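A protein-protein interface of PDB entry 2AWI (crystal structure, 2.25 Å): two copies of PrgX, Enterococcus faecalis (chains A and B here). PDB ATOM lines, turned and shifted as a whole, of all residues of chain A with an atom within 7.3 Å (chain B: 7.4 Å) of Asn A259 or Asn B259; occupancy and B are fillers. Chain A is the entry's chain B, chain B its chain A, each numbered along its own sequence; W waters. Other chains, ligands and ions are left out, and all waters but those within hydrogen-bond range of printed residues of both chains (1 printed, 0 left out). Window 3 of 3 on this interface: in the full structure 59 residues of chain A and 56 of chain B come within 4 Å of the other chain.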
ATOM      1  N   TYR A 238       2.150  29.095   2.441  1.00  0.00           N
ATOM      2  CA  TYR A 238       2.072  28.619   3.812  1.00  0.00           C
ATOM      3  C   TYR A 238       0.837  29.223   4.465  1.00  0.00           C
ATOM      4  O   TYR A 238       0.043  28.524   5.087  1.00  0.00           O
ATOM      5  CB  TYR A 238       3.314  29.030   4.602  1.00  0.00           C
ATOM      6  CG  TYR A 238       3.124  28.964   6.102  1.00  0.00           C
ATOM      7  CD1 TYR A 238       2.604  30.051   6.808  1.00  0.00           C
ATOM      8  CD2 TYR A 238       3.440  27.804   6.815  1.00  0.00           C
ATOM      9  CE1 TYR A 238       2.406  29.988   8.181  1.00  0.00           C
ATOM     10  CE2 TYR A 238       3.244  27.731   8.190  1.00  0.00           C
ATOM     11  CZ  TYR A 238       2.729  28.825   8.863  1.00  0.00           C
ATOM     12  OH  TYR A 238       2.542  28.761  10.220  1.00  0.00           O
ATOM     13  N   SER A 253      -3.983  20.460   5.023  1.00  0.00           N
ATOM     14  CA  SER A 253      -3.513  21.835   4.995  1.00  0.00           C
ATOM     15  C   SER A 253      -2.533  22.092   6.135  1.00  0.00           C
ATOM     16  O   SER A 253      -1.478  22.702   5.938  1.00  0.00           O
ATOM     17  CB  SER A 253      -4.695  22.798   5.105  1.00  0.00           C
ATOM     18  OG  SER A 253      -5.569  22.651   3.998  1.00  0.00           O
ATOM     19  N   TYR A 254      -2.876  21.611   7.324  1.00  0.00           N
ATOM     20  CA  TYR A 254      -2.015  21.818   8.476  1.00  0.00           C
ATOM     21  C   TYR A 254      -0.667  21.141   8.269  1.00  0.00           C
ATOM     22  O   TYR A 254       0.378  21.685   8.645  1.00  0.00           O
ATOM     23  CB  TYR A 254      -2.683  21.282   9.745  1.00  0.00           C
ATOM     24  CG  TYR A 254      -2.003  21.739  11.016  1.00  0.00           C
ATOM     25  CD1 TYR A 254      -0.862  21.094  11.491  1.00  0.00           C
ATOM     26  CD2 TYR A 254      -2.480  22.841  11.727  1.00  0.00           C
ATOM     27  CE1 TYR A 254      -0.214  21.532  12.641  1.00  0.00           C
ATOM     28  CE2 TYR A 254      -1.834  23.293  12.882  1.00  0.00           C
ATOM     29  CZ  TYR A 254      -0.702  22.630  13.329  1.00  0.00           C
ATOM     30  OH  TYR A 254      -0.043  23.062  14.457  1.00  0.00           O
ATOM     31  N   LEU A 255      -0.702  19.952   7.670  1.00  0.00           N
ATOM     32  CA  LEU A 255       0.512  19.189   7.416  1.00  0.00           C
ATOM     33  C   LEU A 255       1.350  19.913   6.378  1.00  0.00           C
ATOM     34  O   LEU A 255       2.579  19.927   6.459  1.00  0.00           O
ATOM     35  CB  LEU A 255       0.173  17.770   6.937  1.00  0.00           C
ATOM     36  CG  LEU A 255      -0.534  16.851   7.948  1.00  0.00           C
ATOM     37  CD1 LEU A 255      -0.756  15.466   7.331  1.00  0.00           C
ATOM     38  CD2 LEU A 255       0.303  16.744   9.224  1.00  0.00           C
ATOM     39  N   ASN A 256       0.685  20.519   5.399  1.00  0.00           N
ATOM     40  CA  ASN A 256       1.397  21.264   4.380  1.00  0.00           C
ATOM     41  C   ASN A 256       2.076  22.465   5.014  1.00  0.00           C
ATOM     42  O   ASN A 256       3.231  22.762   4.715  1.00  0.00           O
ATOM     43  CB  ASN A 256       0.447  21.742   3.286  1.00  0.00           C
ATOM     44  CG  ASN A 256      -0.052  20.611   2.419  1.00  0.00           C
ATOM     45  OD1 ASN A 256       0.685  19.666   2.138  1.00  0.00           O
ATOM     46  ND2 ASN A 256      -1.303  20.708   1.969  1.00  0.00           N
ATOM     47  N   ALA A 257       1.363  23.157   5.896  1.00  0.00           N
ATOM     48  CA  ALA A 257       1.931  24.322   6.550  1.00  0.00           C
ATOM     49  C   ALA A 257       3.198  23.893   7.259  1.00  0.00           C
ATOM     50  O   ALA A 257       4.245  24.522   7.118  1.00  0.00           O
ATOM     51  CB  ALA A 257       0.943  24.906   7.546  1.00  0.00           C
ATOM     52  N   VAL A 258       3.095  22.810   8.018  1.00  0.00           N
ATOM     53  CA  VAL A 258       4.232  22.291   8.762  1.00  0.00           C
ATOM     54  C   VAL A 258       5.390  21.950   7.826  1.00  0.00           C
ATOM     55  O   VAL A 258       6.541  22.305   8.088  1.00  0.00           O
ATOM     56  CB  VAL A 258       3.849  21.016   9.560  1.00  0.00           C
ATOM     57  CG1 VAL A 258       5.054  20.520  10.341  1.00  0.00           C
ATOM     58  CG2 VAL A 258       2.692  21.309  10.514  1.00  0.00           C
ATOM     59  N   ASN A 259       5.083  21.266   6.730  1.00  0.00           N
ATOM     60  CA  ASN A 259       6.114  20.879   5.784  1.00  0.00           C
ATOM     61  C   ASN A 259       6.843  22.095   5.224  1.00  0.00           C
ATOM     62  O   ASN A 259       8.079  22.127   5.174  1.00  0.00           O
ATOM     63  CB  ASN A 259       5.513  20.047   4.649  1.00  0.00           C
ATOM     64  CG  ASN A 259       6.576  19.455   3.741  1.00  0.00           C
ATOM     65  OD1 ASN A 259       7.690  19.150   4.184  1.00  0.00           O
ATOM     66  ND2 ASN A 259       6.236  19.273   2.470  1.00  0.00           N
ATOM     67  N   ILE A 260       6.081  23.099   4.806  1.00  0.00           N
ATOM     68  CA  ILE A 260       6.685  24.307   4.269  1.00  0.00           C
ATOM     69  C   ILE A 260       7.649  24.937   5.277  1.00  0.00           C
ATOM     70  O   ILE A 260       8.651  25.541   4.891  1.00  0.00           O
ATOM     71  CB  ILE A 260       5.605  25.320   3.855  1.00  0.00           C
ATOM     72  CG1 ILE A 260       4.966  24.856   2.539  1.00  0.00           C
ATOM     73  CG2 ILE A 260       6.211  26.712   3.733  1.00  0.00           C
ATOM     74  CD1 ILE A 260       3.831  25.727   2.063  1.00  0.00           C
ATOM     75  N   ILE A 261       7.344  24.790   6.564  1.00  0.00           N
ATOM     76  CA  ILE A 261       8.207  25.325   7.611  1.00  0.00           C
ATOM     77  C   ILE A 261       9.502  24.525   7.603  1.00  0.00           C
ATOM     78  O   ILE A 261      10.588  25.073   7.793  1.00  0.00           O
ATOM     79  CB  ILE A 261       7.547  25.215   9.012  1.00  0.00           C
ATOM     80  CG1 ILE A 261       6.459  26.280   9.153  1.00  0.00           C
ATOM     81  CG2 ILE A 261       8.596  25.374  10.109  1.00  0.00           C
ATOM     82  CD1 ILE A 261       5.859  26.369  10.542  1.00  0.00           C
ATOM     83  N   ASN A 262       9.373  23.221   7.375  1.00  0.00           N
ATOM     84  CA  ASN A 262      10.522  22.328   7.328  1.00  0.00           C
ATOM     85  C   ASN A 262      11.450  22.732   6.185  1.00  0.00           C
ATOM     86  O   ASN A 262      12.670  22.791   6.350  1.00  0.00           O
ATOM     87  CB  ASN A 262      10.057  20.878   7.141  1.00  0.00           C
ATOM     88  CG  ASN A 262      11.213  19.920   6.895  1.00  0.00           C
ATOM     89  OD1 ASN A 262      12.145  19.832   7.698  1.00  0.00           O
ATOM     90  ND2 ASN A 262      11.156  19.194   5.781  1.00  0.00           N
ATOM     91  N   ILE A 263      10.866  23.016   5.027  1.00  0.00           N
ATOM     92  CA  ILE A 263      11.644  23.427   3.868  1.00  0.00           C
ATOM     93  C   ILE A 263      12.500  24.662   4.145  1.00  0.00           C
ATOM     94  O   ILE A 263      13.681  24.694   3.789  1.00  0.00           O
ATOM     95  CB  ILE A 263      10.733  23.716   2.678  1.00  0.00           C
ATOM     96  CG1 ILE A 263      10.090  22.415   2.205  1.00  0.00           C
ATOM     97  CG2 ILE A 263      11.523  24.336   1.553  1.00  0.00           C
ATOM     98  CD1 ILE A 263      11.083  21.381   1.703  1.00  0.00           C
ATOM     99  N   PHE A 264      11.910  25.676   4.773  1.00  0.00           N
ATOM    100  CA  PHE A 264      12.648  26.894   5.074  1.00  0.00           C
ATOM    101  C   PHE A 264      13.830  26.578   5.968  1.00  0.00           C
ATOM    102  O   PHE A 264      14.861  27.244   5.898  1.00  0.00           O
ATOM    103  CB  PHE A 264      11.740  27.935   5.736  1.00  0.00           C
ATOM    104  CG  PHE A 264      10.896  28.716   4.757  1.00  0.00           C
ATOM    105  CD1 PHE A 264      11.485  29.607   3.864  1.00  0.00           C
ATOM    106  CD2 PHE A 264       9.513  28.564   4.729  1.00  0.00           C
ATOM    107  CE1 PHE A 264      10.710  30.335   2.961  1.00  0.00           C
ATOM    108  CE2 PHE A 264       8.729  29.287   3.830  1.00  0.00           C
ATOM    109  CZ  PHE A 264       9.331  30.173   2.948  1.00  0.00           C
ATOM    110  N   LYS A 265      13.678  25.559   6.808  1.00  0.00           N
ATOM    111  CA  LYS A 265      14.747  25.134   7.703  1.00  0.00           C
ATOM    112  C   LYS A 265      15.793  24.382   6.873  1.00  0.00           C
ATOM    113  O   LYS A 265      16.992  24.616   6.993  1.00  0.00           O
ATOM    114  CB  LYS A 265      14.184  24.214   8.786  1.00  0.00           C
ATOM    115  CG  LYS A 265      15.233  23.618   9.713  1.00  0.00           C
ATOM    116  CD  LYS A 265      14.606  22.631  10.694  1.00  0.00           C
ATOM    117  CE  LYS A 265      13.934  21.466   9.962  1.00  0.00           C
ATOM    118  NZ  LYS A 265      13.208  20.528  10.867  1.00  0.00           N
ATOM    119  N   ILE A 266      15.319  23.484   6.020  1.00  0.00           N
ATOM    120  CA  ILE A 266      16.197  22.705   5.162  1.00  0.00           C
ATOM    121  C   ILE A 266      17.100  23.575   4.288  1.00  0.00           C
ATOM    122  O   ILE A 266      18.305  23.338   4.223  1.00  0.00           O
ATOM    123  CB  ILE A 266      15.370  21.759   4.258  1.00  0.00           C
ATOM    124  CG1 ILE A 266      14.857  20.581   5.091  1.00  0.00           C
ATOM    125  CG2 ILE A 266      16.201  21.300   3.063  1.00  0.00           C
ATOM    126  CD1 ILE A 266      14.039  19.577   4.307  1.00  0.00           C
ATOM    127  N   GLU A 294       7.667  18.221  16.233  1.00  0.00           N
ATOM    128  CA  GLU A 294       8.724  18.972  15.576  1.00  0.00           C
ATOM    129  C   GLU A 294       8.785  20.446  15.978  1.00  0.00           C
ATOM    130  O   GLU A 294       9.799  20.911  16.506  1.00  0.00           O
ATOM    131  CB  GLU A 294       8.540  18.860  14.058  1.00  0.00           C
ATOM    132  CG  GLU A 294       9.454  19.751  13.234  1.00  0.00           C
ATOM    133  CD  GLU A 294       9.037  19.819  11.773  1.00  0.00           C
ATOM    134  OE1 GLU A 294       9.060  18.769  11.091  1.00  0.00           O
ATOM    135  OE2 GLU A 294       8.684  20.927  11.308  1.00  0.00           O
ATOM    136  N   TYR B 238      18.074  21.312  -3.716  1.00  0.00           N
ATOM    137  CA  TYR B 238      17.611  19.973  -4.040  1.00  0.00           C
ATOM    138  C   TYR B 238      18.756  19.236  -4.742  1.00  0.00           C
ATOM    139  O   TYR B 238      18.935  18.034  -4.562  1.00  0.00           O
ATOM    140  CB  TYR B 238      16.378  20.036  -4.952  1.00  0.00           C
ATOM    141  CG  TYR B 238      16.278  18.897  -5.949  1.00  0.00           C
ATOM    142  CD1 TYR B 238      16.818  19.014  -7.226  1.00  0.00           C
ATOM    143  CD2 TYR B 238      15.670  17.694  -5.604  1.00  0.00           C
ATOM    144  CE1 TYR B 238      16.756  17.961  -8.137  1.00  0.00           C
ATOM    145  CE2 TYR B 238      15.604  16.633  -6.504  1.00  0.00           C
ATOM    146  CZ  TYR B 238      16.150  16.773  -7.768  1.00  0.00           C
ATOM    147  OH  TYR B 238      16.091  15.725  -8.660  1.00  0.00           O
ATOM    148  N   ASP B 252      18.283  10.266   4.212  1.00  0.00           N
ATOM    149  CA  ASP B 252      17.681  11.546   4.587  1.00  0.00           C
ATOM    150  C   ASP B 252      17.858  12.564   3.467  1.00  0.00           C
ATOM    151  O   ASP B 252      16.977  13.397   3.231  1.00  0.00           O
ATOM    152  CB  ASP B 252      18.295  12.107   5.874  1.00  0.00           C
ATOM    153  CG  ASP B 252      17.756  11.432   7.119  1.00  0.00           C
ATOM    154  OD1 ASP B 252      16.619  10.913   7.070  1.00  0.00           O
ATOM    155  OD2 ASP B 252      18.459  11.433   8.148  1.00  0.00           O
ATOM    156  N   SER B 253      18.994  12.497   2.779  1.00  0.00           N
ATOM    157  CA  SER B 253      19.251  13.416   1.680  1.00  0.00           C
ATOM    158  C   SER B 253      18.326  13.091   0.523  1.00  0.00           C
ATOM    159  O   SER B 253      17.910  13.982  -0.223  1.00  0.00           O
ATOM    160  CB  SER B 253      20.702  13.313   1.211  1.00  0.00           C
ATOM    161  OG  SER B 253      21.586  13.840   2.182  1.00  0.00           O
ATOM    162  N   TYR B 254      18.004  11.812   0.372  1.00  0.00           N
ATOM    163  CA  TYR B 254      17.127  11.398  -0.708  1.00  0.00           C
ATOM    164  C   TYR B 254      15.714  11.869  -0.413  1.00  0.00           C
ATOM    165  O   TYR B 254      14.995  12.300  -1.309  1.00  0.00           O
ATOM    166  CB  TYR B 254      17.147   9.879  -0.870  1.00  0.00           C
ATOM    167  CG  TYR B 254      16.483   9.405  -2.142  1.00  0.00           C
ATOM    168  CD1 TYR B 254      15.092   9.321  -2.241  1.00  0.00           C
ATOM    169  CD2 TYR B 254      17.249   9.084  -3.263  1.00  0.00           C
ATOM    170  CE1 TYR B 254      14.482   8.930  -3.435  1.00  0.00           C
ATOM    171  CE2 TYR B 254      16.652   8.695  -4.457  1.00  0.00           C
ATOM    172  CZ  TYR B 254      15.272   8.622  -4.537  1.00  0.00           C
ATOM    173  OH  TYR B 254      14.696   8.261  -5.724  1.00  0.00           O
ATOM    174  N   LEU B 255      15.327  11.783   0.853  1.00  0.00           N
ATOM    175  CA  LEU B 255      14.008  12.217   1.280  1.00  0.00           C
ATOM    176  C   LEU B 255      13.890  13.737   1.149  1.00  0.00           C
ATOM    177  O   LEU B 255      12.879  14.240   0.659  1.00  0.00           O
ATOM    178  CB  LEU B 255      13.759  11.793   2.727  1.00  0.00           C
ATOM    179  CG  LEU B 255      13.883  10.287   2.984  1.00  0.00           C
ATOM    180  CD1 LEU B 255      13.550   9.989   4.443  1.00  0.00           C
ATOM    181  CD2 LEU B 255      12.945   9.523   2.050  1.00  0.00           C
ATOM    182  N   ASN B 256      14.920  14.463   1.582  1.00  0.00           N
ATOM    183  CA  ASN B 256      14.906  15.919   1.485  1.00  0.00           C
ATOM    184  C   ASN B 256      14.653  16.328   0.033  1.00  0.00           C
ATOM    185  O   ASN B 256      13.818  17.188  -0.246  1.00  0.00           O
ATOM    186  CB  ASN B 256      16.237  16.517   1.961  1.00  0.00           C
ATOM    187  CG  ASN B 256      16.440  16.402   3.470  1.00  0.00           C
ATOM    188  OD1 ASN B 256      15.483  16.326   4.237  1.00  0.00           O
ATOM    189  ND2 ASN B 256      17.696  16.416   3.901  1.00  0.00           N
ATOM    190  N   ALA B 257      15.374  15.694  -0.889  1.00  0.00           N
ATOM    191  CA  ALA B 257      15.227  15.988  -2.308  1.00  0.00           C
ATOM    192  C   ALA B 257      13.802  15.723  -2.767  1.00  0.00           C
ATOM    193  O   ALA B 257      13.210  16.554  -3.454  1.00  0.00           O
ATOM    194  CB  ALA B 257      16.206  15.155  -3.127  1.00  0.00           C
ATOM    195  N   VAL B 258      13.254  14.569  -2.395  1.00  0.00           N
ATOM    196  CA  VAL B 258      11.888  14.223  -2.787  1.00  0.00           C
ATOM    197  C   VAL B 258      10.912  15.232  -2.180  1.00  0.00           C
ATOM    198  O   VAL B 258       9.944  15.653  -2.818  1.00  0.00           O
ATOM    199  CB  VAL B 258      11.495  12.794  -2.304  1.00  0.00           C
ATOM    200  CG1 VAL B 258      10.079  12.449  -2.774  1.00  0.00           C
ATOM    201  CG2 VAL B 258      12.486  11.759  -2.840  1.00  0.00           C
ATOM    202  N   ASN B 259      11.187  15.630  -0.946  1.00  0.00           N
ATOM    203  CA  ASN B 259      10.340  16.578  -0.250  1.00  0.00           C
ATOM    204  C   ASN B 259      10.361  17.948  -0.935  1.00  0.00           C
ATOM    205  O   ASN B 259       9.354  18.667  -0.960  1.00  0.00           O
ATOM    206  CB  ASN B 259      10.792  16.689   1.201  1.00  0.00           C
ATOM    207  CG  ASN B 259       9.899  17.581   2.013  1.00  0.00           C
ATOM    208  OD1 ASN B 259       8.681  17.592   1.832  1.00  0.00           O
ATOM    209  ND2 ASN B 259      10.495  18.333   2.928  1.00  0.00           N
ATOM    210  N   ILE B 260      11.507  18.304  -1.503  1.00  0.00           N
ATOM    211  CA  ILE B 260      11.611  19.573  -2.197  1.00  0.00           C
ATOM    212  C   ILE B 260      10.822  19.506  -3.508  1.00  0.00           C
ATOM    213  O   ILE B 260      10.134  20.463  -3.873  1.00  0.00           O
ATOM    214  CB  ILE B 260      13.085  19.935  -2.449  1.00  0.00           C
ATOM    215  CG1 ILE B 260      13.734  20.307  -1.108  1.00  0.00           C
ATOM    216  CG2 ILE B 260      13.196  21.080  -3.454  1.00  0.00           C
ATOM    217  CD1 ILE B 260      15.168  20.737  -1.210  1.00  0.00           C
ATOM    218  N   ILE B 261      10.906  18.374  -4.206  1.00  0.00           N
ATOM    219  CA  ILE B 261      10.164  18.202  -5.454  1.00  0.00           C
ATOM    220  C   ILE B 261       8.679  18.393  -5.144  1.00  0.00           C
ATOM    221  O   ILE B 261       7.936  18.983  -5.927  1.00  0.00           O
ATOM    222  CB  ILE B 261      10.376  16.790  -6.053  1.00  0.00           C
ATOM    223  CG1 ILE B 261      11.812  16.653  -6.565  1.00  0.00           C
ATOM    224  CG2 ILE B 261       9.392  16.541  -7.194  1.00  0.00           C
ATOM    225  CD1 ILE B 261      12.094  15.332  -7.250  1.00  0.00           C
ATOM    226  N   ASN B 262       8.260  17.899  -3.986  1.00  0.00           N
ATOM    227  CA  ASN B 262       6.874  18.006  -3.561  1.00  0.00           C
ATOM    228  C   ASN B 262       6.452  19.449  -3.273  1.00  0.00           C
ATOM    229  O   ASN B 262       5.307  19.823  -3.520  1.00  0.00           O
ATOM    230  CB  ASN B 262       6.642  17.140  -2.325  1.00  0.00           C
ATOM    231  CG  ASN B 262       5.273  17.352  -1.717  1.00  0.00           C
ATOM    232  OD1 ASN B 262       4.252  17.186  -2.385  1.00  0.00           O
ATOM    233  ND2 ASN B 262       5.245  17.722  -0.440  1.00  0.00           N
ATOM    234  N   ILE B 263       7.370  20.254  -2.743  1.00  0.00           N
ATOM    235  CA  ILE B 263       7.067  21.652  -2.447  1.00  0.00           C
ATOM    236  C   ILE B 263       6.728  22.404  -3.730  1.00  0.00           C
ATOM    237  O   ILE B 263       5.790  23.206  -3.763  1.00  0.00           O
ATOM    238  CB  ILE B 263       8.258  22.346  -1.755  1.00  0.00           C
ATOM    239  CG1 ILE B 263       8.243  22.016  -0.266  1.00  0.00           C
ATOM    240  CG2 ILE B 263       8.192  23.838  -1.955  1.00  0.00           C
ATOM    241  CD1 ILE B 263       6.954  22.427   0.434  1.00  0.00           C
ATOM    242  N   PHE B 264       7.491  22.139  -4.784  1.00  0.00           N
ATOM    243  CA  PHE B 264       7.265  22.791  -6.063  1.00  0.00           C
ATOM    244  C   PHE B 264       5.876  22.452  -6.576  1.00  0.00           C
ATOM    245  O   PHE B 264       5.255  23.245  -7.281  1.00  0.00           O
ATOM    246  CB  PHE B 264       8.335  22.360  -7.087  1.00  0.00           C
ATOM    247  CG  PHE B 264       9.632  23.120  -6.962  1.00  0.00           C
ATOM    248  CD1 PHE B 264       9.678  24.492  -7.227  1.00  0.00           C
ATOM    249  CD2 PHE B 264      10.795  22.482  -6.540  1.00  0.00           C
ATOM    250  CE1 PHE B 264      10.866  25.220  -7.067  1.00  0.00           C
ATOM    251  CE2 PHE B 264      11.990  23.201  -6.376  1.00  0.00           C
ATOM    252  CZ  PHE B 264      12.024  24.571  -6.640  1.00  0.00           C
ATOM    253  N   LYS B 265       5.393  21.264  -6.229  1.00  0.00           N
ATOM    254  CA  LYS B 265       4.072  20.848  -6.659  1.00  0.00           C
ATOM    255  C   LYS B 265       3.034  21.671  -5.912  1.00  0.00           C
ATOM    256  O   LYS B 265       2.132  22.249  -6.513  1.00  0.00           O
ATOM    257  CB  LYS B 265       3.842  19.366  -6.361  1.00  0.00           C
ATOM    258  CG  LYS B 265       2.480  18.857  -6.834  1.00  0.00           C
ATOM    259  CD  LYS B 265       2.085  17.541  -6.169  1.00  0.00           C
ATOM    260  CE  LYS B 265       1.865  17.715  -4.665  1.00  0.00           C
ATOM    261  NZ  LYS B 265       1.381  16.473  -3.982  1.00  0.00           N
ATOM    262  N   ILE B 266       3.176  21.724  -4.595  1.00  0.00           N
ATOM    263  CA  ILE B 266       2.249  22.459  -3.750  1.00  0.00           C
ATOM    264  C   ILE B 266       2.081  23.923  -4.148  1.00  0.00           C
ATOM    265  O   ILE B 266       0.960  24.387  -4.343  1.00  0.00           O
ATOM    266  CB  ILE B 266       2.686  22.400  -2.274  1.00  0.00           C
ATOM    267  CG1 ILE B 266       2.770  20.944  -1.813  1.00  0.00           C
ATOM    268  CG2 ILE B 266       1.687  23.144  -1.407  1.00  0.00           C
ATOM    269  CD1 ILE B 266       3.146  20.786  -0.352  1.00  0.00           C
ATOM    270  N   LEU B 280      15.227  13.307 -11.131  1.00  0.00           N
ATOM    271  CA  LEU B 280      15.388  12.309 -10.079  1.00  0.00           C
ATOM    272  C   LEU B 280      15.151  10.877 -10.561  1.00  0.00           C
ATOM    273  O   LEU B 280      15.708   9.930 -10.006  1.00  0.00           O
ATOM    274  CB  LEU B 280      14.449  12.620  -8.910  1.00  0.00           C
ATOM    275  CG  LEU B 280      14.537  11.678  -7.706  1.00  0.00           C
ATOM    276  CD1 LEU B 280      15.928  11.760  -7.091  1.00  0.00           C
ATOM    277  CD2 LEU B 280      13.479  12.049  -6.684  1.00  0.00           C
ATOM    278  N   GLU B 294       5.340   8.119  -5.451  1.00  0.00           N
ATOM    279  CA  GLU B 294       4.985   9.471  -5.845  1.00  0.00           C
ATOM    280  C   GLU B 294       5.591   9.861  -7.188  1.00  0.00           C
ATOM    281  O   GLU B 294       4.892   9.931  -8.200  1.00  0.00           O
ATOM    282  CB  GLU B 294       5.461  10.434  -4.756  1.00  0.00           C
ATOM    283  CG  GLU B 294       5.352  11.902  -5.089  1.00  0.00           C
ATOM    284  CD  GLU B 294       5.996  12.765  -4.024  1.00  0.00           C
ATOM    285  OE1 GLU B 294       5.574  12.667  -2.850  1.00  0.00           O
ATOM    286  OE2 GLU B 294       6.925  13.537  -4.357  1.00  0.00           O
HETATM  287  O   HOH W   1      12.721  16.672   4.163  1.00  0.00           O
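Water W1 lies within hydrogen-bond range of the side-chain amide oxygen of Asn B256 (2.8 Å), the side-chain amide nitrogen of Asn B259 (3.0 Å) and the side-chain amide nitrogen of Asn A262 (3.4 Å).
Asn A256 touches Ile B266, and with the chains exchanged Ile A266 touches Asn B256.
Asn A259 touches Ile B263, and with the chains exchanged Ile A263 touches Asn B259.
Ile A260 touches Ile B263, but with the chains exchanged Ile A263 does not touch Ile B260 (4.01 Å).
Ile A263 touches its own counterpart, Ile B263.
ND2 of Asn B256 sits close to O of Asp B252, at 3.2 Å.
NZ of Lys B265 lies close to OD1 of Asn B262, 3.4 Å away.
OD1 of Asn A262 sits close to NZ of Lys A265.
The side-chain amide nitrogen (ND2) of Asn B259 lies close to the side-chain amide nitrogen (ND2) of Asn A262, 3.1 Å away.
The side-chain amide oxygen (OD1) of Asn A259 lies close to the side-chain amide oxygen (OD1) of Asn B259 (3.0 Å).
The side-chain amide nitrogen (ND2) of Asn A259 sits close to the side-chain amide nitrogen (ND2) of Asn B262 (3.4 Å).
OD1 of Asn A256 touches CD1 of Ile B266, at 3.7 Å.
ND2 of Asn A259 touches CD1 of Ile B263, 3.8 Å away.
CD1 of Ile B263 touches CG1 of Ile A260, at 3.8 Å.
Ile A263 touches Asn B259 (CD1 to ND2, 3.3 Å).
Ile A263 touches Ile B263.
Ile A266 touches Asn B256.
Asn A259 touches just these residues of chain B: Asn B259 (3.0 Å), Asn B262 (3.4 Å) and Ile B263 (3.8 Å).
Printed residues of chain B within 4 Å of Ile A266: Asn B256.
Tyr B238 touches none of the printed residues of chain A.
Printed residues of chain A within 4 Å of Asn B259: Asn A259, Asn A262 and Ile A263.
Printed residues of chain A within 4 Å of Ile B263: Asn A259, Ile A260 and Ile A263.
Glu B294 touches none of the printed residues of chain A.
The nearest residue of chain B that does not touch Asn A259 is Ile B266 (4.4 Å).
The nearest printed residue of chain A that does not touch Asn B259 is Ile A266 (4.001 Å).
Hydrophobic or aromatic side chains of chain B within 4 Å of the printed part of chain A: Ile B263 and Ile B266.
Among the printed residues, 9 pairs touch across the chains.
Among the printed residues, no Asp or Glu carboxylate lies within 4 Å of a Lys or Arg side-chain nitrogen of the other chain.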
